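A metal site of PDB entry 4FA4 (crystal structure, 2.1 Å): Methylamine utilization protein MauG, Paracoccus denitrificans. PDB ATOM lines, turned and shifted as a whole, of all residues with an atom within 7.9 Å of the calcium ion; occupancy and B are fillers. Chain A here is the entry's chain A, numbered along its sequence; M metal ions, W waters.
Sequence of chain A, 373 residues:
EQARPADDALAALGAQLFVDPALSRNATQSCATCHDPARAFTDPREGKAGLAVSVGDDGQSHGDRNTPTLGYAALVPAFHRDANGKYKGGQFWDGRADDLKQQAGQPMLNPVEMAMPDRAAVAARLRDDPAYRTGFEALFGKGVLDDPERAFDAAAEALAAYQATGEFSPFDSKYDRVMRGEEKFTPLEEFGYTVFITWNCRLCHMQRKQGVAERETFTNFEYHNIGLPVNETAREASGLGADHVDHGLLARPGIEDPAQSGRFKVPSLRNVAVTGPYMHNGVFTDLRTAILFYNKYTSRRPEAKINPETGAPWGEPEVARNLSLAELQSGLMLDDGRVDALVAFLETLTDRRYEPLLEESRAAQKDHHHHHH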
ATOM      1  N   ARG A  39      21.314  13.203  -7.361  1.00  0.00           N
ATOM      2  CA  ARG A  39      19.962  13.448  -6.900  1.00  0.00           C
ATOM      3  C   ARG A  39      19.031  13.933  -8.000  1.00  0.00           C
ATOM      4  O   ARG A  39      18.201  14.825  -7.777  1.00  0.00           O
ATOM      5  CB  ARG A  39      19.954  14.441  -5.767  1.00  0.00           C
ATOM      6  CG  ARG A  39      18.604  14.570  -5.130  1.00  0.00           C
ATOM      7  CD  ARG A  39      18.696  15.479  -3.935  1.00  0.00           C
ATOM      8  NE  ARG A  39      17.416  15.634  -3.268  1.00  0.00           N
ATOM      9  CZ  ARG A  39      16.993  14.868  -2.277  1.00  0.00           C
ATOM     10  NH1 ARG A  39      17.750  13.865  -1.838  1.00  0.00           N
ATOM     11  NH2 ARG A  39      15.802  15.104  -1.724  1.00  0.00           N
ATOM     12  N   THR A  42      18.983  17.755  -8.689  1.00  0.00           N
ATOM     13  CA  THR A  42      18.393  18.711  -7.727  1.00  0.00           C
ATOM     14  C   THR A  42      19.340  18.846  -6.545  1.00  0.00           C
ATOM     15  O   THR A  42      20.425  18.232  -6.543  1.00  0.00           O
ATOM     16  CB  THR A  42      16.986  18.286  -7.247  1.00  0.00           C
ATOM     17  OG1 THR A  42      17.086  17.060  -6.521  1.00  0.00           O
ATOM     18  CG2 THR A  42      16.040  18.101  -8.379  1.00  0.00           C
ATOM     19  N   ASP A  43      18.909  19.597  -5.511  1.00  0.00           N
ATOM     20  CA  ASP A  43      19.817  20.079  -4.497  1.00  0.00           C
ATOM     21  C   ASP A  43      19.618  19.354  -3.193  1.00  0.00           C
ATOM     22  O   ASP A  43      18.569  19.599  -2.486  1.00  0.00           O
ATOM     23  CB  ASP A  43      19.761  21.608  -4.334  1.00  0.00           C
ATOM     24  CG  ASP A  43      20.938  22.164  -3.428  1.00  0.00           C
ATOM     25  OD1 ASP A  43      21.080  23.414  -3.260  1.00  0.00           O
ATOM     26  OD2 ASP A  43      21.728  21.353  -2.912  1.00  0.00           O
ATOM     27  N   LEU A  51      15.269  21.719   2.441  1.00  0.00           N
ATOM     28  CA  LEU A  51      15.619  21.498   1.039  1.00  0.00           C
ATOM     29  C   LEU A  51      14.703  22.249   0.083  1.00  0.00           C
ATOM     30  O   LEU A  51      14.806  22.075  -1.123  1.00  0.00           O
ATOM     31  CB  LEU A  51      15.613  19.994   0.708  1.00  0.00           C
ATOM     32  CG  LEU A  51      16.868  19.126   0.883  1.00  0.00           C
ATOM     33  CD1 LEU A  51      17.855  19.734   1.790  1.00  0.00           C
ATOM     34  CD2 LEU A  51      16.454  17.768   1.380  1.00  0.00           C
ATOM     35  N   ALA A  52      13.847  23.111   0.619  1.00  0.00           N
ATOM     36  CA  ALA A  52      12.903  23.897  -0.163  1.00  0.00           C
ATOM     37  C   ALA A  52      13.608  24.823  -1.126  1.00  0.00           C
ATOM     38  O   ALA A  52      13.164  24.950  -2.256  1.00  0.00           O
ATOM     39  CB  ALA A  52      11.921  24.678   0.724  1.00  0.00           C
ATOM     40  N   ASN A  66      12.396  26.340  -5.347  1.00  0.00           N
ATOM     41  CA  ASN A  66      12.986  25.024  -5.271  1.00  0.00           C
ATOM     42  C   ASN A  66      13.707  24.721  -6.587  1.00  0.00           C
ATOM     43  O   ASN A  66      13.235  25.093  -7.712  1.00  0.00           O
ATOM     44  CB  ASN A  66      11.870  24.020  -5.056  1.00  0.00           C
ATOM     45  CG  ASN A  66      12.371  22.605  -4.928  1.00  0.00           C
ATOM     46  OD1 ASN A  66      11.983  21.688  -5.731  1.00  0.00           O
ATOM     47  ND2 ASN A  66      13.212  22.382  -3.896  1.00  0.00           N
ATOM     48  N   THR A  67      14.864  24.114  -6.444  1.00  0.00           N
ATOM     49  CA  THR A  67      15.706  23.771  -7.555  1.00  0.00           C
ATOM     50  C   THR A  67      15.058  22.583  -8.270  1.00  0.00           C
ATOM     51  O   THR A  67      14.906  21.507  -7.692  1.00  0.00           O
ATOM     52  CB  THR A  67      17.151  23.502  -7.068  1.00  0.00           C
ATOM     53  OG1 THR A  67      17.708  24.714  -6.521  1.00  0.00           O
ATOM     54  CG2 THR A  67      18.031  22.977  -8.237  1.00  0.00           C
ATOM     55  N   PRO A  68      14.613  22.782  -9.532  1.00  0.00           N
ATOM     56  CA  PRO A  68      14.074  21.672 -10.289  1.00  0.00           C
ATOM     57  C   PRO A  68      15.148  20.745 -10.912  1.00  0.00           C
ATOM     58  O   PRO A  68      16.318  21.107 -11.164  1.00  0.00           O
ATOM     59  CB  PRO A  68      13.235  22.359 -11.379  1.00  0.00           C
ATOM     60  CG  PRO A  68      14.002  23.591 -11.661  1.00  0.00           C
ATOM     61  CD  PRO A  68      14.573  24.034 -10.314  1.00  0.00           C
ATOM     62  N   THR A  69      14.725  19.535 -11.161  1.00  0.00           N
ATOM     63  CA  THR A  69      15.498  18.631 -11.925  1.00  0.00           C
ATOM     64  C   THR A  69      15.815  19.209 -13.301  1.00  0.00           C
ATOM     65  O   THR A  69      15.054  20.028 -13.862  1.00  0.00           O
ATOM     66  CB  THR A  69      14.715  17.392 -12.143  1.00  0.00           C
ATOM     67  OG1 THR A  69      15.569  16.463 -12.790  1.00  0.00           O
ATOM     68  CG2 THR A  69      13.396  17.736 -13.022  1.00  0.00           C
ATOM     69  N   TRP A  93      10.414  27.922 -13.402  1.00  0.00           N
ATOM     70  CA  TRP A  93       9.058  27.747 -12.926  1.00  0.00           C
ATOM     71  C   TRP A  93       8.110  28.799 -13.463  1.00  0.00           C
ATOM     72  O   TRP A  93       6.916  28.539 -13.571  1.00  0.00           O
ATOM     73  CB  TRP A  93       9.039  27.818 -11.413  1.00  0.00           C
ATOM     74  CG  TRP A  93       9.599  26.683 -10.685  1.00  0.00           C
ATOM     75  CD1 TRP A  93      10.807  26.644 -10.066  1.00  0.00           C
ATOM     76  CD2 TRP A  93       8.972  25.409 -10.435  1.00  0.00           C
ATOM     77  NE1 TRP A  93      10.975  25.432  -9.429  1.00  0.00           N
ATOM     78  CE2 TRP A  93       9.866  24.654  -9.643  1.00  0.00           C
ATOM     79  CE3 TRP A  93       7.732  24.841 -10.779  1.00  0.00           C
ATOM     80  CZ2 TRP A  93       9.551  23.333  -9.181  1.00  0.00           C
ATOM     81  CZ3 TRP A  93       7.437  23.522 -10.340  1.00  0.00           C
ATOM     82  CH2 TRP A  93       8.332  22.804  -9.547  1.00  0.00           C
ATOM     83  N   ASN A 271      11.001  11.359 -12.473  1.00  0.00           N
ATOM     84  CA  ASN A 271      11.828  11.420 -11.271  1.00  0.00           C
ATOM     85  C   ASN A 271      11.169  12.127 -10.069  1.00  0.00           C
ATOM     86  O   ASN A 271      11.854  12.422  -9.115  1.00  0.00           O
ATOM     87  CB  ASN A 271      13.199  12.067 -11.563  1.00  0.00           C
ATOM     88  CG  ASN A 271      14.081  11.217 -12.438  1.00  0.00           C
ATOM     89  OD1 ASN A 271      14.103  10.014 -12.300  1.00  0.00           O
ATOM     90  ND2 ASN A 271      14.824  11.853 -13.378  1.00  0.00           N
ATOM     91  N   VAL A 272       9.880  12.462 -10.174  1.00  0.00           N
ATOM     92  CA  VAL A 272       9.210  13.191  -9.105  1.00  0.00           C
ATOM     93  C   VAL A 272       9.452  12.518  -7.765  1.00  0.00           C
ATOM     94  O   VAL A 272       9.591  13.201  -6.735  1.00  0.00           O
ATOM     95  CB  VAL A 272       7.678  13.452  -9.374  1.00  0.00           C
ATOM     96  CG1 VAL A 272       6.818  12.171  -9.312  1.00  0.00           C
ATOM     97  CG2 VAL A 272       7.138  14.516  -8.495  1.00  0.00           C
ATOM     98  N   VAL A 274      11.890  11.354  -6.416  1.00  0.00           N
ATOM     99  CA  VAL A 274      13.160  11.541  -5.769  1.00  0.00           C
ATOM    100  C   VAL A 274      13.632  12.999  -5.759  1.00  0.00           C
ATOM    101  O   VAL A 274      14.779  13.280  -5.426  1.00  0.00           O
ATOM    102  CB  VAL A 274      14.254  10.578  -6.393  1.00  0.00           C
ATOM    103  CG1 VAL A 274      13.783   9.152  -6.328  1.00  0.00           C
ATOM    104  CG2 VAL A 274      14.549  10.941  -7.813  1.00  0.00           C
ATOM    105  N   THR A 275      12.775  13.959  -6.155  1.00  0.00           N
ATOM    106  CA  THR A 275      13.196  15.356  -6.178  1.00  0.00           C
ATOM    107  C   THR A 275      12.365  16.193  -5.202  1.00  0.00           C
ATOM    108  O   THR A 275      12.122  17.382  -5.434  1.00  0.00           O
ATOM    109  CB  THR A 275      13.072  15.905  -7.572  1.00  0.00           C
ATOM    110  OG1 THR A 275      11.705  15.736  -7.970  1.00  0.00           O
ATOM    111  CG2 THR A 275      13.984  15.151  -8.512  1.00  0.00           C
ATOM    112  N   GLY A 276      11.904  15.571  -4.118  1.00  0.00           N
ATOM    113  CA  GLY A 276      11.375  16.308  -2.944  1.00  0.00           C
ATOM    114  C   GLY A 276      12.320  17.408  -2.506  1.00  0.00           C
ATOM    115  O   GLY A 276      13.536  17.290  -2.713  1.00  0.00           O
ATOM    116  N   PRO A 277      11.797  18.489  -1.887  1.00  0.00           N
ATOM    117  CA  PRO A 277      10.411  18.706  -1.694  1.00  0.00           C
ATOM    118  C   PRO A 277       9.718  19.239  -2.984  1.00  0.00           C
ATOM    119  O   PRO A 277      10.325  19.316  -4.071  1.00  0.00           O
ATOM    120  CB  PRO A 277      10.374  19.729  -0.550  1.00  0.00           C
ATOM    121  CG  PRO A 277      11.567  20.485  -0.750  1.00  0.00           C
ATOM    122  CD  PRO A 277      12.584  19.524  -1.187  1.00  0.00           C
ATOM    123  N   TYR A 278       8.442  19.559  -2.865  1.00  0.00           N
ATOM    124  CA  TYR A 278       7.628  19.728  -4.061  1.00  0.00           C
ATOM    125  C   TYR A 278       7.107  21.142  -4.239  1.00  0.00           C
ATOM    126  O   TYR A 278       7.156  21.987  -3.312  1.00  0.00           O
ATOM    127  CB  TYR A 278       6.518  18.650  -4.135  1.00  0.00           C
ATOM    128  CG  TYR A 278       7.147  17.274  -4.165  1.00  0.00           C
ATOM    129  CD1 TYR A 278       7.266  16.504  -2.995  1.00  0.00           C
ATOM    130  CD2 TYR A 278       7.738  16.792  -5.301  1.00  0.00           C
ATOM    131  CE1 TYR A 278       7.876  15.289  -3.007  1.00  0.00           C
ATOM    132  CE2 TYR A 278       8.338  15.555  -5.317  1.00  0.00           C
ATOM    133  CZ  TYR A 278       8.407  14.823  -4.180  1.00  0.00           C
ATOM    134  OH  TYR A 278       9.037  13.594  -4.191  1.00  0.00           O
ATOM    135  N   MET A 279       6.673  21.367  -5.470  1.00  0.00           N
ATOM    136  CA  MET A 279       6.087  22.618  -5.964  1.00  0.00           C
ATOM    137  C   MET A 279       7.153  23.647  -6.112  1.00  0.00           C
ATOM    138  O   MET A 279       8.317  23.428  -5.686  1.00  0.00           O
ATOM    139  CB  MET A 279       4.932  23.090  -5.091  1.00  0.00           C
ATOM    140  CG  MET A 279       3.805  22.039  -4.947  1.00  0.00           C
ATOM    141  SD  MET A 279       3.020  21.396  -6.439  1.00  0.00           S
ATOM    142  CE  MET A 279       1.959  20.122  -5.702  1.00  0.00           C
ATOM    143  N   HIS A 280       6.755  24.785  -6.677  1.00  0.00           N
ATOM    144  CA  HIS A 280       7.679  25.829  -7.061  1.00  0.00           C
ATOM    145  C   HIS A 280       8.469  26.345  -5.835  1.00  0.00           C
ATOM    146  O   HIS A 280       9.561  26.860  -5.974  1.00  0.00           O
ATOM    147  CB  HIS A 280       6.918  26.940  -7.817  1.00  0.00           C
ATOM    148  CG  HIS A 280       5.986  27.746  -6.949  1.00  0.00           C
ATOM    149  ND1 HIS A 280       4.614  27.595  -6.963  1.00  0.00           N
ATOM    150  CD2 HIS A 280       6.235  28.712  -6.023  1.00  0.00           C
ATOM    151  CE1 HIS A 280       4.062  28.427  -6.105  1.00  0.00           C
ATOM    152  NE2 HIS A 280       5.025  29.138  -5.542  1.00  0.00           N
ATOM    153  N   ASN A 281       7.903  26.197  -4.652  1.00  0.00           N
ATOM    154  CA  ASN A 281       8.503  26.801  -3.459  1.00  0.00           C
ATOM    155  C   ASN A 281       9.017  25.732  -2.498  1.00  0.00           C
ATOM    156  O   ASN A 281       9.384  26.053  -1.387  1.00  0.00           O
ATOM    157  CB  ASN A 281       7.551  27.818  -2.760  1.00  0.00           C
ATOM    158  CG  ASN A 281       6.180  27.205  -2.430  1.00  0.00           C
ATOM    159  OD1 ASN A 281       6.020  26.008  -2.449  1.00  0.00           O
ATOM    160  ND2 ASN A 281       5.190  28.045  -2.132  1.00  0.00           N
ATOM    161  N   GLY A 282       9.051  24.484  -2.927  1.00  0.00           N
ATOM    162  CA  GLY A 282       9.384  23.385  -2.023  1.00  0.00           C
ATOM    163  C   GLY A 282       8.448  23.234  -0.826  1.00  0.00           C
ATOM    164  O   GLY A 282       8.796  22.573   0.138  1.00  0.00           O
ATOM    165  N   PHE A 284       5.915  21.377   0.065  1.00  0.00           N
ATOM    166  CA  PHE A 284       5.569  20.025   0.517  1.00  0.00           C
ATOM    167  C   PHE A 284       6.771  19.089   0.431  1.00  0.00           C
ATOM    168  O   PHE A 284       7.335  18.892  -0.670  1.00  0.00           O
ATOM    169  CB  PHE A 284       4.414  19.426  -0.297  1.00  0.00           C
ATOM    170  CG  PHE A 284       3.259  20.379  -0.472  1.00  0.00           C
ATOM    171  CD1 PHE A 284       2.658  20.970   0.633  1.00  0.00           C
ATOM    172  CD2 PHE A 284       2.785  20.679  -1.736  1.00  0.00           C
ATOM    173  CE1 PHE A 284       1.623  21.849   0.489  1.00  0.00           C
ATOM    174  CE2 PHE A 284       1.710  21.549  -1.885  1.00  0.00           C
ATOM    175  CZ  PHE A 284       1.130  22.145  -0.753  1.00  0.00           C
HETATM  176 CA    CA M   1      11.542  19.484  -5.975  1.00  0.00          CA
HETATM  177  O   HOH W   1      13.239  19.563  -7.787  1.00  0.00           O
HETATM  178  O   HOH W   2      10.411  18.050  -7.411  1.00  0.00           O
HETATM  179  O   HOH W   3       9.850  20.881  -6.949  1.00  0.00           O
HETATM  180  O   HOH W   4      13.392  19.561  -4.446  1.00  0.00           O
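Within 4 Å of the calcium ion: Asn 66, Thr 275 and Pro 277.
NE1 of Trp 93 is in hydrogen-bond range of O of Asn 66 (2.9 Å).
The backbone carbonyl oxygen (O) of Leu 51 is in hydrogen-bond range of the side-chain amide nitrogen (ND2) of Asn 66, at 3.2 Å.
ND2 of Asn 66 sits close to O of Ala 52 (3.0 Å).
The backbone NH (N) of Asn 66 is in hydrogen-bond range of the backbone carbonyl oxygen (O) of His 280 (2.9 Å).
The calcium ion is bound by O of Thr 275 (2.2 Å), OD1 of Asn 66 (2.3 Å), O of Pro 277 (2.3 Å), water W2 (2.3 Å), water W3 (2.4 Å), water W4 (2.4 Å) and water W1 (2.5 Å).
The calcium ion has seven donor atoms within binding distance.
Water W4 bridges O of Gly 276 (2.9 Å) and ND2 of Asn 66 (2.9 Å).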
